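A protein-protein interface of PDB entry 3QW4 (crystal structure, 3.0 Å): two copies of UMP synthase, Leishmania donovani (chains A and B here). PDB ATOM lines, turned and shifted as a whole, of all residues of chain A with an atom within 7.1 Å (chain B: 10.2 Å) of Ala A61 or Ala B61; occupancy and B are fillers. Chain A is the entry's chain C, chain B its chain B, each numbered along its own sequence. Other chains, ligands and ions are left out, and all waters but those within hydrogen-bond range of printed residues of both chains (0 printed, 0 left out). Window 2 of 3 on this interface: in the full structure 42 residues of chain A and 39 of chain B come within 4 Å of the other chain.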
ATOM      1  N   ALA A  28       9.764 -18.893   8.917  1.00  0.00           N
ATOM      2  CA  ALA A  28      10.149 -20.130   9.597  1.00  0.00           C
ATOM      3  C   ALA A  28      10.489 -19.871  11.061  1.00  0.00           C
ATOM      4  O   ALA A  28      10.184 -20.693  11.924  1.00  0.00           O
ATOM      5  CB  ALA A  28      11.324 -20.779   8.885  1.00  0.00           C
ATOM      6  N   PHE A  56       5.536 -27.072   8.077  1.00  0.00           N
ATOM      7  CA  PHE A  56       6.966 -26.891   8.255  1.00  0.00           C
ATOM      8  C   PHE A  56       7.695 -27.022   6.919  1.00  0.00           C
ATOM      9  O   PHE A  56       8.593 -26.242   6.603  1.00  0.00           O
ATOM     10  CB  PHE A  56       7.487 -27.919   9.248  1.00  0.00           C
ATOM     11  CG  PHE A  56       6.919 -27.767  10.636  1.00  0.00           C
ATOM     12  CD1 PHE A  56       7.429 -26.808  11.514  1.00  0.00           C
ATOM     13  CD2 PHE A  56       5.890 -28.594  11.076  1.00  0.00           C
ATOM     14  CE1 PHE A  56       6.920 -26.673  12.802  1.00  0.00           C
ATOM     15  CE2 PHE A  56       5.375 -28.467  12.363  1.00  0.00           C
ATOM     16  CZ  PHE A  56       5.894 -27.502  13.226  1.00  0.00           C
ATOM     17  N   GLU A  57       7.284 -28.008   6.132  1.00  0.00           N
ATOM     18  CA  GLU A  57       7.833 -28.243   4.809  1.00  0.00           C
ATOM     19  C   GLU A  57       7.521 -27.072   3.888  1.00  0.00           C
ATOM     20  O   GLU A  57       8.150 -26.899   2.846  1.00  0.00           O
ATOM     21  CB  GLU A  57       7.226 -29.518   4.248  1.00  0.00           C
ATOM     22  CG  GLU A  57       8.099 -30.228   3.254  1.00  0.00           C
ATOM     23  CD  GLU A  57       7.459 -31.488   2.717  1.00  0.00           C
ATOM     24  OE1 GLU A  57       7.568 -31.697   1.488  1.00  0.00           O
ATOM     25  OE2 GLU A  57       6.849 -32.260   3.506  1.00  0.00           O
ATOM     26  N   PHE A  58       6.536 -26.276   4.288  1.00  0.00           N
ATOM     27  CA  PHE A  58       6.164 -25.068   3.575  1.00  0.00           C
ATOM     28  C   PHE A  58       7.361 -24.134   3.447  1.00  0.00           C
ATOM     29  O   PHE A  58       7.550 -23.490   2.409  1.00  0.00           O
ATOM     30  CB  PHE A  58       5.011 -24.356   4.296  1.00  0.00           C
ATOM     31  CG  PHE A  58       4.414 -23.212   3.517  1.00  0.00           C
ATOM     32  CD1 PHE A  58       4.899 -21.915   3.671  1.00  0.00           C
ATOM     33  CD2 PHE A  58       3.367 -23.429   2.634  1.00  0.00           C
ATOM     34  CE1 PHE A  58       4.351 -20.846   2.953  1.00  0.00           C
ATOM     35  CE2 PHE A  58       2.814 -22.369   1.914  1.00  0.00           C
ATOM     36  CZ  PHE A  58       3.308 -21.072   2.076  1.00  0.00           C
ATOM     37  N   PHE A  59       8.176 -24.080   4.499  1.00  0.00           N
ATOM     38  CA  PHE A  59       9.268 -23.115   4.570  1.00  0.00           C
ATOM     39  C   PHE A  59      10.568 -23.604   3.940  1.00  0.00           C
ATOM     40  O   PHE A  59      11.614 -22.971   4.093  1.00  0.00           O
ATOM     41  CB  PHE A  59       9.484 -22.647   6.015  1.00  0.00           C
ATOM     42  CG  PHE A  59       8.264 -22.050   6.637  1.00  0.00           C
ATOM     43  CD1 PHE A  59       7.723 -20.866   6.140  1.00  0.00           C
ATOM     44  CD2 PHE A  59       7.646 -22.678   7.708  1.00  0.00           C
ATOM     45  CE1 PHE A  59       6.583 -20.322   6.704  1.00  0.00           C
ATOM     46  CE2 PHE A  59       6.507 -22.139   8.282  1.00  0.00           C
ATOM     47  CZ  PHE A  59       5.973 -20.960   7.781  1.00  0.00           C
ATOM     48  N   GLY A  60      10.498 -24.721   3.222  1.00  0.00           N
ATOM     49  CA  GLY A  60      11.655 -25.246   2.516  1.00  0.00           C
ATOM     50  C   GLY A  60      12.742 -25.743   3.446  1.00  0.00           C
ATOM     51  O   GLY A  60      12.464 -26.447   4.424  1.00  0.00           O
ATOM     52  N   ALA A  61      13.981 -25.370   3.132  1.00  0.00           N
ATOM     53  CA  ALA A  61      15.157 -25.787   3.908  1.00  0.00           C
ATOM     54  C   ALA A  61      15.124 -25.281   5.349  1.00  0.00           C
ATOM     55  O   ALA A  61      15.383 -26.046   6.287  1.00  0.00           O
ATOM     56  CB  ALA A  61      16.434 -25.342   3.218  1.00  0.00           C
ATOM     57  N   GLU A  62      14.800 -23.996   5.509  1.00  0.00           N
ATOM     58  CA  GLU A  62      14.649 -23.378   6.830  1.00  0.00           C
ATOM     59  C   GLU A  62      13.501 -24.014   7.610  1.00  0.00           C
ATOM     60  O   GLU A  62      13.504 -24.017   8.840  1.00  0.00           O
ATOM     61  CB  GLU A  62      14.431 -21.864   6.705  1.00  0.00           C
ATOM     62  N   GLY A  63      12.530 -24.561   6.884  1.00  0.00           N
ATOM     63  CA  GLY A  63      11.387 -25.232   7.497  1.00  0.00           C
ATOM     64  C   GLY A  63      11.711 -26.590   8.087  1.00  0.00           C
ATOM     65  O   GLY A  63      11.050 -27.044   9.013  1.00  0.00           O
ATOM     66  N   TRP A  64      12.732 -27.240   7.548  1.00  0.00           N
ATOM     67  CA  TRP A  64      13.120 -28.547   8.043  1.00  0.00           C
ATOM     68  C   TRP A  64      13.925 -28.489   9.320  1.00  0.00           C
ATOM     69  O   TRP A  64      13.732 -29.309  10.222  1.00  0.00           O
ATOM     70  CB  TRP A  64      13.839 -29.334   6.963  1.00  0.00           C
ATOM     71  CG  TRP A  64      12.911 -30.322   6.392  1.00  0.00           C
ATOM     72  CD1 TRP A  64      11.999 -30.117   5.391  1.00  0.00           C
ATOM     73  CD2 TRP A  64      12.743 -31.674   6.823  1.00  0.00           C
ATOM     74  NE1 TRP A  64      11.288 -31.271   5.157  1.00  0.00           N
ATOM     75  CE2 TRP A  64      11.724 -32.244   6.022  1.00  0.00           C
ATOM     76  CE3 TRP A  64      13.364 -32.467   7.799  1.00  0.00           C
ATOM     77  CZ2 TRP A  64      11.304 -33.577   6.172  1.00  0.00           C
ATOM     78  CZ3 TRP A  64      12.950 -33.792   7.944  1.00  0.00           C
ATOM     79  CH2 TRP A  64      11.928 -34.333   7.129  1.00  0.00           C
ATOM     80  N   ALA A  65      14.822 -27.507   9.385  1.00  0.00           N
ATOM     81  CA  ALA A  65      15.588 -27.233  10.584  1.00  0.00           C
ATOM     82  C   ALA A  65      14.653 -26.724  11.664  1.00  0.00           C
ATOM     83  O   ALA A  65      14.921 -26.892  12.852  1.00  0.00           O
ATOM     84  CB  ALA A  65      16.672 -26.218  10.294  1.00  0.00           C
ATOM     85  N   ALA A  66      13.550 -26.114  11.234  1.00  0.00           N
ATOM     86  CA  ALA A  66      12.527 -25.597  12.141  1.00  0.00           C
ATOM     87  C   ALA A  66      11.734 -26.721  12.804  1.00  0.00           C
ATOM     88  O   ALA A  66      11.438 -26.654  13.994  1.00  0.00           O
ATOM     89  CB  ALA A  66      11.589 -24.648  11.397  1.00  0.00           C
ATOM     90  N   ALA B  28      24.427 -34.796   1.406  1.00  0.00           N
ATOM     91  CA  ALA B  28      23.447 -34.113   0.548  1.00  0.00           C
ATOM     92  C   ALA B  28      24.099 -33.436  -0.658  1.00  0.00           C
ATOM     93  O   ALA B  28      23.482 -33.297  -1.701  1.00  0.00           O
ATOM     94  CB  ALA B  28      22.646 -33.097   1.357  1.00  0.00           C
ATOM     95  N   ALA B  29      25.348 -33.006  -0.499  1.00  0.00           N
ATOM     96  CA  ALA B  29      26.097 -32.356  -1.575  1.00  0.00           C
ATOM     97  C   ALA B  29      26.450 -33.345  -2.694  1.00  0.00           C
ATOM     98  O   ALA B  29      26.400 -32.994  -3.882  1.00  0.00           O
ATOM     99  CB  ALA B  29      27.352 -31.691  -1.011  1.00  0.00           C
ATOM    100  N   VAL B  32      23.269 -34.076  -4.921  1.00  0.00           N
ATOM    101  CA  VAL B  32      23.111 -33.092  -5.984  1.00  0.00           C
ATOM    102  C   VAL B  32      24.095 -33.378  -7.118  1.00  0.00           C
ATOM    103  O   VAL B  32      23.715 -33.388  -8.284  1.00  0.00           O
ATOM    104  CB  VAL B  32      23.323 -31.660  -5.473  1.00  0.00           C
ATOM    105  CG1 VAL B  32      22.990 -30.647  -6.550  1.00  0.00           C
ATOM    106  CG2 VAL B  32      22.477 -31.407  -4.263  1.00  0.00           C
ATOM    107  N   PHE B  55      14.472 -39.505  -0.405  1.00  0.00           N
ATOM    108  CA  PHE B  55      15.922 -39.595  -0.407  1.00  0.00           C
ATOM    109  C   PHE B  55      16.566 -38.242  -0.224  1.00  0.00           C
ATOM    110  O   PHE B  55      17.711 -38.153   0.224  1.00  0.00           O
ATOM    111  CB  PHE B  55      16.417 -40.286  -1.677  1.00  0.00           C
ATOM    112  CG  PHE B  55      15.799 -41.635  -1.889  1.00  0.00           C
ATOM    113  CD1 PHE B  55      14.629 -41.770  -2.652  1.00  0.00           C
ATOM    114  CD2 PHE B  55      16.361 -42.771  -1.298  1.00  0.00           C
ATOM    115  CE1 PHE B  55      14.034 -43.019  -2.835  1.00  0.00           C
ATOM    116  CE2 PHE B  55      15.777 -44.025  -1.476  1.00  0.00           C
ATOM    117  CZ  PHE B  55      14.604 -44.151  -2.245  1.00  0.00           C
ATOM    118  N   PHE B  56      15.822 -37.194  -0.557  1.00  0.00           N
ATOM    119  CA  PHE B  56      16.299 -35.836  -0.352  1.00  0.00           C
ATOM    120  C   PHE B  56      15.962 -35.420   1.057  1.00  0.00           C
ATOM    121  O   PHE B  56      16.681 -34.640   1.677  1.00  0.00           O
ATOM    122  CB  PHE B  56      15.672 -34.877  -1.366  1.00  0.00           C
ATOM    123  CG  PHE B  56      16.102 -35.137  -2.769  1.00  0.00           C
ATOM    124  CD1 PHE B  56      17.193 -34.473  -3.303  1.00  0.00           C
ATOM    125  CD2 PHE B  56      15.435 -36.064  -3.551  1.00  0.00           C
ATOM    126  CE1 PHE B  56      17.606 -34.728  -4.604  1.00  0.00           C
ATOM    127  CE2 PHE B  56      15.837 -36.325  -4.842  1.00  0.00           C
ATOM    128  CZ  PHE B  56      16.923 -35.659  -5.373  1.00  0.00           C
ATOM    129  N   GLU B  57      14.861 -35.970   1.557  1.00  0.00           N
ATOM    130  CA  GLU B  57      14.356 -35.663   2.893  1.00  0.00           C
ATOM    131  C   GLU B  57      15.226 -36.330   3.954  1.00  0.00           C
ATOM    132  O   GLU B  57      15.249 -35.899   5.108  1.00  0.00           O
ATOM    133  CB  GLU B  57      12.914 -36.138   3.021  1.00  0.00           C
ATOM    134  CG  GLU B  57      11.939 -35.051   3.385  1.00  0.00           C
ATOM    135  CD  GLU B  57      10.491 -35.547   3.378  1.00  0.00           C
ATOM    136  OE1 GLU B  57      10.050 -36.065   4.437  1.00  0.00           O
ATOM    137  OE2 GLU B  57       9.800 -35.446   2.319  1.00  0.00           O
ATOM    138  N   PHE B  58      15.934 -37.377   3.535  1.00  0.00           N
ATOM    139  CA  PHE B  58      16.883 -38.090   4.367  1.00  0.00           C
ATOM    140  C   PHE B  58      17.911 -37.159   5.002  1.00  0.00           C
ATOM    141  O   PHE B  58      18.285 -37.334   6.169  1.00  0.00           O
ATOM    142  CB  PHE B  58      17.604 -39.138   3.527  1.00  0.00           C
ATOM    143  CG  PHE B  58      18.302 -40.188   4.338  1.00  0.00           C
ATOM    144  CD1 PHE B  58      19.657 -40.054   4.659  1.00  0.00           C
ATOM    145  CD2 PHE B  58      17.604 -41.318   4.777  1.00  0.00           C
ATOM    146  CE1 PHE B  58      20.310 -41.035   5.410  1.00  0.00           C
ATOM    147  CE2 PHE B  58      18.243 -42.304   5.530  1.00  0.00           C
ATOM    148  CZ  PHE B  58      19.601 -42.163   5.846  1.00  0.00           C
ATOM    149  N   PHE B  59      18.360 -36.171   4.235  1.00  0.00           N
ATOM    150  CA  PHE B  59      19.406 -35.249   4.688  1.00  0.00           C
ATOM    151  C   PHE B  59      18.874 -33.961   5.325  1.00  0.00           C
ATOM    152  O   PHE B  59      19.612 -32.981   5.465  1.00  0.00           O
ATOM    153  CB  PHE B  59      20.331 -34.894   3.528  1.00  0.00           C
ATOM    154  CG  PHE B  59      20.908 -36.088   2.812  1.00  0.00           C
ATOM    155  CD1 PHE B  59      22.027 -36.749   3.314  1.00  0.00           C
ATOM    156  CD2 PHE B  59      20.351 -36.532   1.623  1.00  0.00           C
ATOM    157  CE1 PHE B  59      22.568 -37.837   2.643  1.00  0.00           C
ATOM    158  CE2 PHE B  59      20.893 -37.618   0.950  1.00  0.00           C
ATOM    159  CZ  PHE B  59      21.997 -38.268   1.462  1.00  0.00           C
ATOM    160  N   GLY B  60      17.599 -33.957   5.693  1.00  0.00           N
ATOM    161  CA  GLY B  60      17.010 -32.831   6.400  1.00  0.00           C
ATOM    162  C   GLY B  60      17.181 -31.489   5.714  1.00  0.00           C
ATOM    163  O   GLY B  60      16.828 -31.335   4.549  1.00  0.00           O
ATOM    164  N   ALA B  61      17.739 -30.525   6.445  1.00  0.00           N
ATOM    165  CA  ALA B  61      17.766 -29.119   6.026  1.00  0.00           C
ATOM    166  C   ALA B  61      18.499 -28.917   4.705  1.00  0.00           C
ATOM    167  O   ALA B  61      17.920 -28.411   3.732  1.00  0.00           O
ATOM    168  CB  ALA B  61      18.362 -28.233   7.133  1.00  0.00           C
ATOM    169  N   GLU B  62      19.766 -29.328   4.673  1.00  0.00           N
ATOM    170  CA  GLU B  62      20.551 -29.291   3.443  1.00  0.00           C
ATOM    171  C   GLU B  62      19.883 -30.116   2.326  1.00  0.00           C
ATOM    172  O   GLU B  62      19.948 -29.751   1.147  1.00  0.00           O
ATOM    173  CB  GLU B  62      21.984 -29.769   3.702  1.00  0.00           C
ATOM    174  N   GLY B  63      19.225 -31.210   2.715  1.00  0.00           N
ATOM    175  CA  GLY B  63      18.578 -32.112   1.777  1.00  0.00           C
ATOM    176  C   GLY B  63      17.486 -31.459   0.964  1.00  0.00           C
ATOM    177  O   GLY B  63      17.330 -31.736  -0.218  1.00  0.00           O
ATOM    178  N   TRP B  64      16.723 -30.585   1.593  1.00  0.00           N
ATOM    179  CA  TRP B  64      15.632 -29.926   0.902  1.00  0.00           C
ATOM    180  C   TRP B  64      16.162 -28.924  -0.134  1.00  0.00           C
ATOM    181  O   TRP B  64      15.689 -28.878  -1.271  1.00  0.00           O
ATOM    182  CB  TRP B  64      14.720 -29.250   1.910  1.00  0.00           C
ATOM    183  CG  TRP B  64      13.350 -29.040   1.407  1.00  0.00           C
ATOM    184  CD1 TRP B  64      12.256 -29.820   1.673  1.00  0.00           C
ATOM    185  CD2 TRP B  64      12.892 -27.977   0.548  1.00  0.00           C
ATOM    186  NE1 TRP B  64      11.140 -29.308   1.033  1.00  0.00           N
ATOM    187  CE2 TRP B  64      11.503 -28.178   0.340  1.00  0.00           C
ATOM    188  CE3 TRP B  64      13.518 -26.872  -0.062  1.00  0.00           C
ATOM    189  CZ2 TRP B  64      10.725 -27.306  -0.453  1.00  0.00           C
ATOM    190  CZ3 TRP B  64      12.746 -26.010  -0.859  1.00  0.00           C
ATOM    191  CH2 TRP B  64      11.365 -26.231  -1.039  1.00  0.00           C
ATOM    192  N   ALA B  65      17.155 -28.129   0.258  1.00  0.00           N
ATOM    193  CA  ALA B  65      17.802 -27.213  -0.671  1.00  0.00           C
ATOM    194  C   ALA B  65      18.467 -27.994  -1.808  1.00  0.00           C
ATOM    195  O   ALA B  65      18.689 -27.459  -2.897  1.00  0.00           O
ATOM    196  CB  ALA B  65      18.807 -26.350   0.055  1.00  0.00           C
ATOM    197  N   ALA B  66      18.772 -29.263  -1.541  1.00  0.00           N
ATOM    198  CA  ALA B  66      19.323 -30.167  -2.541  1.00  0.00           C
ATOM    199  C   ALA B  66      18.256 -30.585  -3.559  1.00  0.00           C
ATOM    200  O   ALA B  66      18.532 -30.683  -4.754  1.00  0.00           O
ATOM    201  CB  ALA B  66      19.941 -31.387  -1.868  1.00  0.00           C
ATOM    202  N   LEU B  67      17.036 -30.812  -3.080  1.00  0.00           N
ATOM    203  CA  LEU B  67      15.910 -31.160  -3.949  1.00  0.00           C
ATOM    204  C   LEU B  67      15.574 -30.030  -4.907  1.00  0.00           C
ATOM    205  O   LEU B  67      15.344 -30.243  -6.099  1.00  0.00           O
ATOM    206  CB  LEU B  67      14.681 -31.513  -3.113  1.00  0.00           C
ATOM    207  CG  LEU B  67      13.354 -31.812  -3.804  1.00  0.00           C
ATOM    208  CD1 LEU B  67      13.452 -33.001  -4.738  1.00  0.00           C
ATOM    209  CD2 LEU B  67      12.311 -32.068  -2.736  1.00  0.00           C
ATOM    210  N   SER B  68      15.563 -28.824  -4.363  1.00  0.00           N
ATOM    211  CA  SER B  68      15.315 -27.622  -5.128  1.00  0.00           C
ATOM    212  C   SER B  68      16.388 -27.393  -6.188  1.00  0.00           C
ATOM    213  O   SER B  68      16.100 -26.875  -7.264  1.00  0.00           O
ATOM    214  CB  SER B  68      15.269 -26.432  -4.185  1.00  0.00           C
ATOM    215  OG  SER B  68      15.255 -25.235  -4.924  1.00  0.00           O
ATOM    216  N   GLU B  69      17.621 -27.777  -5.870  1.00  0.00           N
ATOM    217  CA  GLU B  69      18.750 -27.586  -6.775  1.00  0.00           C
ATOM    218  C   GLU B  69      18.677 -28.598  -7.908  1.00  0.00           C
ATOM    219  O   GLU B  69      18.875 -28.263  -9.073  1.00  0.00           O
ATOM    220  CB  GLU B  69      20.077 -27.712  -6.011  1.00  0.00           C
ATOM    221  CG  GLU B  69      21.272 -26.983  -6.645  1.00  0.00           C
ATOM    222  N   ARG B  72      15.955 -27.595 -10.443  1.00  0.00           N
ATOM    223  CA  ARG B  72      16.347 -26.467 -11.284  1.00  0.00           C
ATOM    224  C   ARG B  72      17.521 -26.790 -12.228  1.00  0.00           C
ATOM    225  O   ARG B  72      17.849 -26.016 -13.140  1.00  0.00           O
ATOM    226  CB  ARG B  72      16.649 -25.250 -10.422  1.00  0.00           C
ATOM    227  CG  ARG B  72      15.430 -24.657  -9.734  1.00  0.00           C
ATOM    228  CD  ARG B  72      15.791 -23.484  -8.800  1.00  0.00           C
ATOM    229  NE  ARG B  72      16.597 -23.910  -7.652  1.00  0.00           N
ATOM    230  CZ  ARG B  72      17.772 -23.384  -7.305  1.00  0.00           C
ATOM    231  NH1 ARG B  72      18.296 -22.379  -8.004  1.00  0.00           N
ATOM    232  NH2 ARG B  72      18.421 -23.861  -6.241  1.00  0.00           N
ATOM    233  N   SER B  99       3.855 -26.065  -1.926  1.00  0.00           N
ATOM    234  CA  SER B  99       5.238 -26.464  -1.744  1.00  0.00           C
ATOM    235  C   SER B  99       5.794 -27.124  -2.994  1.00  0.00           C
ATOM    236  O   SER B  99       6.900 -26.813  -3.430  1.00  0.00           O
ATOM    237  CB  SER B  99       5.344 -27.417  -0.562  1.00  0.00           C
ATOM    238  OG  SER B  99       6.652 -27.953  -0.438  1.00  0.00           O
ATOM    239  N   HIS B 103       6.891 -23.545  -4.838  1.00  0.00           N
ATOM    240  CA  HIS B 103       8.232 -23.438  -4.244  1.00  0.00           C
ATOM    241  C   HIS B 103       9.234 -24.285  -5.026  1.00  0.00           C
ATOM    242  O   HIS B 103      10.219 -23.773  -5.560  1.00  0.00           O
ATOM    243  CB  HIS B 103       8.263 -23.829  -2.751  1.00  0.00           C
ATOM    244  CG  HIS B 103       7.304 -23.066  -1.890  1.00  0.00           C
ATOM    245  ND1 HIS B 103       6.873 -21.791  -2.193  1.00  0.00           N
ATOM    246  CD2 HIS B 103       6.715 -23.394  -0.715  1.00  0.00           C
ATOM    247  CE1 HIS B 103       6.046 -21.372  -1.252  1.00  0.00           C
ATOM    248  NE2 HIS B 103       5.935 -22.326  -0.342  1.00  0.00           N
ATOM    249  N   LEU B 104       8.966 -25.583  -5.100  1.00  0.00           N
ATOM    250  CA  LEU B 104       9.868 -26.514  -5.743  1.00  0.00           C
ATOM    251  C   LEU B 104       9.792 -26.451  -7.269  1.00  0.00           C
ATOM    252  O   LEU B 104      10.723 -26.891  -7.956  1.00  0.00           O
ATOM    253  CB  LEU B 104       9.570 -27.925  -5.255  1.00  0.00           C
ATOM    254  CG  LEU B 104       9.947 -28.255  -3.809  1.00  0.00           C
ATOM    255  CD1 LEU B 104       9.204 -29.509  -3.345  1.00  0.00           C
ATOM    256  CD2 LEU B 104      11.460 -28.414  -3.664  1.00  0.00           C
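Glu A57 touches Trp B64, and with the chains exchanged Trp A64 touches Glu B57. Gly A60 touches Trp B64, and with the chains exchanged Trp A64 touches Gly B60. Ala A61 touches Trp B64, but with the chains exchanged Trp A64 does not touch Ala B61 (4.04 Å). Trp B64 touches its own counterpart, Trp A64. 12 positions are printed for both chains.
The backbone carbonyl oxygen of Ser B99 sits at hydrogen-bond distance from the backbone NH of Leu B104 (2.9 Å).
NE2 of His B103 sits close to O of Phe A58, at 3.4 Å.
Of the 12 printed residues of chain A, 5 touch a printed residue of chain B. Printed residues of chain A that touch a printed residue of chain B: Glu A57, Phe A58, Gly A60, Ala A61 and Trp A64. Hydrophobic or aromatic side chains of chain B within 4 Å of the printed part of chain A: Ala B61, Trp B64 and His B103. Along chain B the printed residues that touch a printed residue of chain A span positions 57 to 103.
Among the printed residues, pairs that only touch across the chains: Glu A57 with Trp B64, Glu A57 with Ser B99, Gly A60 with Trp B64, Ala A61 with Ala B61, Ala A61 with Trp B64, Trp A64 with Glu B57, Trp A64 with Gly B60 and Trp A64 with Trp B64.
Of the printed residues of chain B, Glu A57 touches Trp B64 (3.9 Å) and Ser B99 (3.8 Å). Of chain B, only Trp B64 (3.6 Å) comes within 4 Å of Gly A60. No residue of chain B comes within 4 Å of Glu A62. No residue of chain B comes within 4 Å of Gly A63. Phe B56 touches none of the printed residues of chain A. Phe B58 touches none of the printed residues of chain A. Of chain A, only Ala A61 comes within 4 Å of Ala B61. Printed residues of chain A within 4 Å of His B103: Phe A58 (3.2 Å). The nearest residue of chain A that does not touch Ala B61 is Trp A64 (4.04 Å).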
